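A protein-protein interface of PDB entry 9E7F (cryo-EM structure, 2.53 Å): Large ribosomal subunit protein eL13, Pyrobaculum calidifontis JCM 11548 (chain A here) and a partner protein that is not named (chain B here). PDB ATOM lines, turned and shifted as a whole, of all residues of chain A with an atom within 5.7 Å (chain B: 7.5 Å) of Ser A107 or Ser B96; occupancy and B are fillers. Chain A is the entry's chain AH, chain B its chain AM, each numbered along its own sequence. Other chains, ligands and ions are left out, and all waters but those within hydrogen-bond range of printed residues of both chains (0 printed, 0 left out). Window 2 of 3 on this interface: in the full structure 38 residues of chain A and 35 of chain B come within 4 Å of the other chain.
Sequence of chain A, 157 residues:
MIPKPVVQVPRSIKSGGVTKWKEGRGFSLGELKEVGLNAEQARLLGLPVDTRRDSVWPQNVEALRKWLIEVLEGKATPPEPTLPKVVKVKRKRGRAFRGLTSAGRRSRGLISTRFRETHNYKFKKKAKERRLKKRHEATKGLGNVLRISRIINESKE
Arg B98 touches Ala A103. Ala A103 touches Gln B99. Gln B99 touches Gly A104. Ser A107 touches Ser B96.
O of Trp B94 sits close to OG of Ser A107, at 3.5 Å.
The backbone carbonyl oxygen (O) of Ala A103 lies within hydrogen-bond range of the side-chain hydroxyl (OG) of Ser A107 (3.2 Å). NE2 of Gln B99 sits at hydrogen-bond distance from OE2 of Glu B103 (3.4 Å).
Of the printed residues of chain B, Ala A103 touches Arg B98 and Gln B99. Of the printed residues of chain B, Gly A104 touches Gln B99. Ser A107 touches just these residues of chain B: Trp B94 (3.5 Å) and Ser B96 (3.7 Å). The nearest printed residue of chain A that does not touch Gln B99 is Ser A107 (4.2 Å).
Of the 8 printed residues of chain A, 3 touch a printed residue of chain B. Hydrophobic or aromatic side chains of chain A that line the printed part of chain B: Ala A103. Among the printed residues, 5 pairs touch across the chains. Among the printed residues, no Asp or Glu carboxylate lies within 4 Å of a Lys or Arg side-chain nitrogen of the other chain.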
ATOM      1  N   SER A 102     -12.631  10.064  20.315  1.00  0.00           N
ATOM      2  CA  SER A 102     -13.209   8.730  20.426  1.00  0.00           C
ATOM      3  C   SER A 102     -13.735   8.233  19.083  1.00  0.00           C
ATOM      4  O   SER A 102     -13.562   7.059  18.738  1.00  0.00           O
ATOM      5  CB  SER A 102     -14.316   8.730  21.476  1.00  0.00           C
ATOM      6  OG  SER A 102     -14.747   7.412  21.750  1.00  0.00           O
ATOM      7  N   ALA A 103     -14.374   9.114  18.311  1.00  0.00           N
ATOM      8  CA  ALA A 103     -14.875   8.727  16.997  1.00  0.00           C
ATOM      9  C   ALA A 103     -13.737   8.368  16.052  1.00  0.00           C
ATOM     10  O   ALA A 103     -13.828   7.388  15.304  1.00  0.00           O
ATOM     11  CB  ALA A 103     -15.724   9.849  16.409  1.00  0.00           C
ATOM     12  N   GLY A 104     -12.656   9.144  16.076  1.00  0.00           N
ATOM     13  CA  GLY A 104     -11.510   8.823  15.243  1.00  0.00           C
ATOM     14  C   GLY A 104     -10.843   7.522  15.641  1.00  0.00           C
ATOM     15  O   GLY A 104     -10.411   6.750  14.784  1.00  0.00           O
ATOM     16  N   ARG A 105     -10.749   7.262  16.946  1.00  0.00           N
ATOM     17  CA  ARG A 105     -10.197   5.994  17.411  1.00  0.00           C
ATOM     18  C   ARG A 105     -11.061   4.822  16.972  1.00  0.00           C
ATOM     19  O   ARG A 105     -10.543   3.773  16.571  1.00  0.00           O
ATOM     20  CB  ARG A 105     -10.067   6.007  18.932  1.00  0.00           C
ATOM     21  CG  ARG A 105      -8.943   6.861  19.458  1.00  0.00           C
ATOM     22  CD  ARG A 105      -8.951   6.859  20.967  1.00  0.00           C
ATOM     23  NE  ARG A 105      -9.010   5.510  21.509  1.00  0.00           N
ATOM     24  CZ  ARG A 105      -7.967   4.699  21.603  1.00  0.00           C
ATOM     25  NH1 ARG A 105      -6.771   5.063  21.176  1.00  0.00           N
ATOM     26  NH2 ARG A 105      -8.128   3.493  22.137  1.00  0.00           N
ATOM     27  N   ARG A 106     -12.382   4.978  17.053  1.00  0.00           N
ATOM     28  CA  ARG A 106     -13.275   3.923  16.594  1.00  0.00           C
ATOM     29  C   ARG A 106     -13.123   3.692  15.099  1.00  0.00           C
ATOM     30  O   ARG A 106     -13.104   2.546  14.643  1.00  0.00           O
ATOM     31  CB  ARG A 106     -14.719   4.269  16.937  1.00  0.00           C
ATOM     32  CG  ARG A 106     -15.703   3.182  16.557  1.00  0.00           C
ATOM     33  CD  ARG A 106     -17.129   3.612  16.816  1.00  0.00           C
ATOM     34  NE  ARG A 106     -17.381   3.848  18.232  1.00  0.00           N
ATOM     35  CZ  ARG A 106     -17.534   2.894  19.138  1.00  0.00           C
ATOM     36  NH1 ARG A 106     -17.480   1.616  18.810  1.00  0.00           N
ATOM     37  NH2 ARG A 106     -17.743   3.232  20.406  1.00  0.00           N
ATOM     38  N   SER A 107     -12.997   4.768  14.321  1.00  0.00           N
ATOM     39  CA  SER A 107     -12.812   4.625  12.881  1.00  0.00           C
ATOM     40  C   SER A 107     -11.481   3.962  12.552  1.00  0.00           C
ATOM     41  O   SER A 107     -11.376   3.219  11.570  1.00  0.00           O
ATOM     42  CB  SER A 107     -12.905   5.987  12.203  1.00  0.00           C
ATOM     43  OG  SER A 107     -14.228   6.476  12.232  1.00  0.00           O
ATOM     44  N   ARG A 108     -10.446   4.230  13.351  1.00  0.00           N
ATOM     45  CA  ARG A 108      -9.152   3.597  13.135  1.00  0.00           C
ATOM     46  C   ARG A 108      -9.109   2.158  13.623  1.00  0.00           C
ATOM     47  O   ARG A 108      -8.228   1.407  13.203  1.00  0.00           O
ATOM     48  CB  ARG A 108      -8.049   4.401  13.815  1.00  0.00           C
ATOM     49  CG  ARG A 108      -7.831   5.759  13.197  1.00  0.00           C
ATOM     50  CD  ARG A 108      -7.145   6.700  14.153  1.00  0.00           C
ATOM     51  NE  ARG A 108      -5.736   6.376  14.307  1.00  0.00           N
ATOM     52  CZ  ARG A 108      -5.004   6.723  15.354  1.00  0.00           C
ATOM     53  NH1 ARG A 108      -5.519   7.407  16.357  1.00  0.00           N
ATOM     54  NH2 ARG A 108      -3.725   6.368  15.396  1.00  0.00           N
ATOM     55  N   GLY A 109     -10.027   1.762  14.494  1.00  0.00           N
ATOM     56  CA  GLY A 109     -10.102   0.388  14.942  1.00  0.00           C
ATOM     57  C   GLY A 109      -9.440   0.101  16.267  1.00  0.00           C
ATOM     58  O   GLY A 109      -9.310  -1.074  16.633  1.00  0.00           O
ATOM     59  N   LEU B  67     -25.959  17.784  10.242  1.00  0.00           N
ATOM     60  CA  LEU B  67     -25.401  17.461   8.942  1.00  0.00           C
ATOM     61  C   LEU B  67     -26.249  16.390   8.278  1.00  0.00           C
ATOM     62  O   LEU B  67     -27.033  15.698   8.926  1.00  0.00           O
ATOM     63  CB  LEU B  67     -23.940  17.011   9.039  1.00  0.00           C
ATOM     64  CG  LEU B  67     -23.489  16.064  10.146  1.00  0.00           C
ATOM     65  CD1 LEU B  67     -23.951  14.650   9.893  1.00  0.00           C
ATOM     66  CD2 LEU B  67     -21.986  16.110  10.249  1.00  0.00           C
ATOM     67  N   ALA B  93     -16.982   6.776   3.126  1.00  0.00           N
ATOM     68  CA  ALA B  93     -15.717   7.229   3.675  1.00  0.00           C
ATOM     69  C   ALA B  93     -15.377   6.462   4.947  1.00  0.00           C
ATOM     70  O   ALA B  93     -16.253   5.955   5.646  1.00  0.00           O
ATOM     71  CB  ALA B  93     -15.760   8.727   3.969  1.00  0.00           C
ATOM     72  N   TRP B  94     -14.080   6.390   5.244  1.00  0.00           N
ATOM     73  CA  TRP B  94     -13.616   5.765   6.475  1.00  0.00           C
ATOM     74  C   TRP B  94     -13.837   6.646   7.695  1.00  0.00           C
ATOM     75  O   TRP B  94     -13.615   6.186   8.817  1.00  0.00           O
ATOM     76  CB  TRP B  94     -12.136   5.406   6.351  1.00  0.00           C
ATOM     77  CG  TRP B  94     -11.890   4.121   5.616  1.00  0.00           C
ATOM     78  CD1 TRP B  94     -12.727   3.512   4.740  1.00  0.00           C
ATOM     79  CD2 TRP B  94     -10.728   3.288   5.705  1.00  0.00           C
ATOM     80  NE1 TRP B  94     -12.165   2.355   4.272  1.00  0.00           N
ATOM     81  CE2 TRP B  94     -10.941   2.189   4.858  1.00  0.00           C
ATOM     82  CE3 TRP B  94      -9.532   3.364   6.426  1.00  0.00           C
ATOM     83  CZ2 TRP B  94     -10.001   1.183   4.694  1.00  0.00           C
ATOM     84  CZ3 TRP B  94      -8.605   2.361   6.270  1.00  0.00           C
ATOM     85  CH2 TRP B  94      -8.844   1.283   5.410  1.00  0.00           C
ATOM     86  N   LYS B  95     -14.246   7.893   7.504  1.00  0.00           N
ATOM     87  CA  LYS B  95     -14.639   8.769   8.594  1.00  0.00           C
ATOM     88  C   LYS B  95     -16.122   8.596   8.884  1.00  0.00           C
ATOM     89  O   LYS B  95     -16.931   8.445   7.967  1.00  0.00           O
ATOM     90  CB  LYS B  95     -14.367  10.227   8.230  1.00  0.00           C
ATOM     91  CG  LYS B  95     -13.090  10.805   8.761  1.00  0.00           C
ATOM     92  CD  LYS B  95     -12.981  12.251   8.340  1.00  0.00           C
ATOM     93  CE  LYS B  95     -11.547  12.722   8.335  1.00  0.00           C
ATOM     94  NZ  LYS B  95     -11.354  13.847   7.390  1.00  0.00           N
ATOM     95  N   SER B  96     -16.477   8.636  10.159  1.00  0.00           N
ATOM     96  CA  SER B  96     -17.878   8.668  10.540  1.00  0.00           C
ATOM     97  C   SER B  96     -18.368  10.109  10.617  1.00  0.00           C
ATOM     98  O   SER B  96     -17.582  11.056  10.674  1.00  0.00           O
ATOM     99  CB  SER B  96     -18.092   7.968  11.875  1.00  0.00           C
ATOM    100  OG  SER B  96     -17.453   8.676  12.912  1.00  0.00           O
ATOM    101  N   TRP B  97     -19.693  10.265  10.619  1.00  0.00           N
ATOM    102  CA  TRP B  97     -20.272  11.603  10.665  1.00  0.00           C
ATOM    103  C   TRP B  97     -20.011  12.287  11.997  1.00  0.00           C
ATOM    104  O   TRP B  97     -20.016  13.519  12.067  1.00  0.00           O
ATOM    105  CB  TRP B  97     -21.774  11.545  10.390  1.00  0.00           C
ATOM    106  CG  TRP B  97     -22.123  11.212   8.980  1.00  0.00           C
ATOM    107  CD1 TRP B  97     -23.033  10.291   8.560  1.00  0.00           C
ATOM    108  CD2 TRP B  97     -21.574  11.799   7.797  1.00  0.00           C
ATOM    109  NE1 TRP B  97     -23.081  10.261   7.193  1.00  0.00           N
ATOM    110  CE2 TRP B  97     -22.195  11.179   6.700  1.00  0.00           C
ATOM    111  CE3 TRP B  97     -20.615  12.787   7.559  1.00  0.00           C
ATOM    112  CZ2 TRP B  97     -21.889  11.515   5.389  1.00  0.00           C
ATOM    113  CZ3 TRP B  97     -20.312  13.112   6.262  1.00  0.00           C
ATOM    114  CH2 TRP B  97     -20.946  12.477   5.191  1.00  0.00           C
ATOM    115  N   ARG B  98     -19.795  11.514  13.062  1.00  0.00           N
ATOM    116  CA  ARG B  98     -19.477  12.111  14.353  1.00  0.00           C
ATOM    117  C   ARG B  98     -18.138  12.834  14.313  1.00  0.00           C
ATOM    118  O   ARG B  98     -18.014  13.954  14.818  1.00  0.00           O
ATOM    119  CB  ARG B  98     -19.483  11.034  15.434  1.00  0.00           C
ATOM    120  CG  ARG B  98     -19.397  11.564  16.845  1.00  0.00           C
ATOM    121  CD  ARG B  98     -20.160  10.681  17.803  1.00  0.00           C
ATOM    122  NE  ARG B  98     -19.495   9.401  17.996  1.00  0.00           N
ATOM    123  CZ  ARG B  98     -18.491   9.197  18.835  1.00  0.00           C
ATOM    124  NH1 ARG B  98     -18.014  10.168  19.591  1.00  0.00           N
ATOM    125  NH2 ARG B  98     -17.952   7.986  18.919  1.00  0.00           N
ATOM    126  N   GLN B  99     -17.125  12.218  13.704  1.00  0.00           N
ATOM    127  CA  GLN B  99     -15.844  12.896  13.536  1.00  0.00           C
ATOM    128  C   GLN B  99     -15.963  14.068  12.573  1.00  0.00           C
ATOM    129  O   GLN B  99     -15.284  15.085  12.739  1.00  0.00           O
ATOM    130  CB  GLN B  99     -14.786  11.912  13.052  1.00  0.00           C
ATOM    131  CG  GLN B  99     -13.372  12.429  13.185  1.00  0.00           C
ATOM    132  CD  GLN B  99     -12.357  11.545  12.498  1.00  0.00           C
ATOM    133  OE1 GLN B  99     -12.471  10.325  12.517  1.00  0.00           O
ATOM    134  NE2 GLN B  99     -11.350  12.159  11.896  1.00  0.00           N
ATOM    135  N   VAL B 100     -16.804  13.934  11.548  1.00  0.00           N
ATOM    136  CA  VAL B 100     -17.058  15.042  10.634  1.00  0.00           C
ATOM    137  C   VAL B 100     -17.728  16.193  11.370  1.00  0.00           C
ATOM    138  O   VAL B 100     -17.379  17.362  11.176  1.00  0.00           O
ATOM    139  CB  VAL B 100     -17.903  14.559   9.442  1.00  0.00           C
ATOM    140  CG1 VAL B 100     -18.361  15.728   8.597  1.00  0.00           C
ATOM    141  CG2 VAL B 100     -17.121  13.572   8.605  1.00  0.00           C
ATOM    142  N   ALA B 101     -18.697  15.881  12.230  1.00  0.00           N
ATOM    143  CA  ALA B 101     -19.372  16.915  13.003  1.00  0.00           C
ATOM    144  C   ALA B 101     -18.424  17.585  13.983  1.00  0.00           C
ATOM    145  O   ALA B 101     -18.549  18.784  14.253  1.00  0.00           O
ATOM    146  CB  ALA B 101     -20.567  16.318  13.740  1.00  0.00           C
ATOM    147  N   GLU B 102     -17.485  16.825  14.548  1.00  0.00           N
ATOM    148  CA  GLU B 102     -16.488  17.416  15.434  1.00  0.00           C
ATOM    149  C   GLU B 102     -15.612  18.410  14.688  1.00  0.00           C
ATOM    150  O   GLU B 102     -15.315  19.494  15.196  1.00  0.00           O
ATOM    151  CB  GLU B 102     -15.620  16.330  16.062  1.00  0.00           C
ATOM    152  CG  GLU B 102     -16.348  15.398  16.991  1.00  0.00           C
ATOM    153  CD  GLU B 102     -15.470  14.265  17.476  1.00  0.00           C
ATOM    154  OE1 GLU B 102     -14.356  14.107  16.942  1.00  0.00           O
ATOM    155  OE2 GLU B 102     -15.889  13.532  18.395  1.00  0.00           O
ATOM    156  N   GLU B 103     -15.182  18.051  13.479  1.00  0.00           N
ATOM    157  CA  GLU B 103     -14.290  18.919  12.722  1.00  0.00           C
ATOM    158  C   GLU B 103     -14.983  20.213  12.315  1.00  0.00           C
ATOM    159  O   GLU B 103     -14.371  21.284  12.337  1.00  0.00           O
ATOM    160  CB  GLU B 103     -13.760  18.178  11.494  1.00  0.00           C
ATOM    161  CG  GLU B 103     -12.735  17.102  11.815  1.00  0.00           C
ATOM    162  CD  GLU B 103     -12.591  16.068  10.712  1.00  0.00           C
ATOM    163  OE1 GLU B 103     -13.467  16.010   9.829  1.00  0.00           O
ATOM    164  OE2 GLU B 103     -11.605  15.308  10.730  1.00  0.00           O
ATOM    165  N   PHE B 129     -25.500  16.103  16.356  1.00  0.00           N
ATOM    166  CA  PHE B 129     -24.474  15.768  17.327  1.00  0.00           C
ATOM    167  C   PHE B 129     -24.261  16.951  18.255  1.00  0.00           C
ATOM    168  O   PHE B 129     -24.568  18.093  17.914  1.00  0.00           O
ATOM    169  CB  PHE B 129     -23.150  15.401  16.653  1.00  0.00           C
ATOM    170  CG  PHE B 129     -23.246  14.246  15.709  1.00  0.00           C
ATOM    171  CD1 PHE B 129     -23.115  12.951  16.168  1.00  0.00           C
ATOM    172  CD2 PHE B 129     -23.460  14.453  14.360  1.00  0.00           C
ATOM    173  CE1 PHE B 129     -23.200  11.894  15.305  1.00  0.00           C
ATOM    174  CE2 PHE B 129     -23.544  13.395  13.497  1.00  0.00           C
ATOM    175  CZ  PHE B 129     -23.410  12.116  13.969  1.00  0.00           C
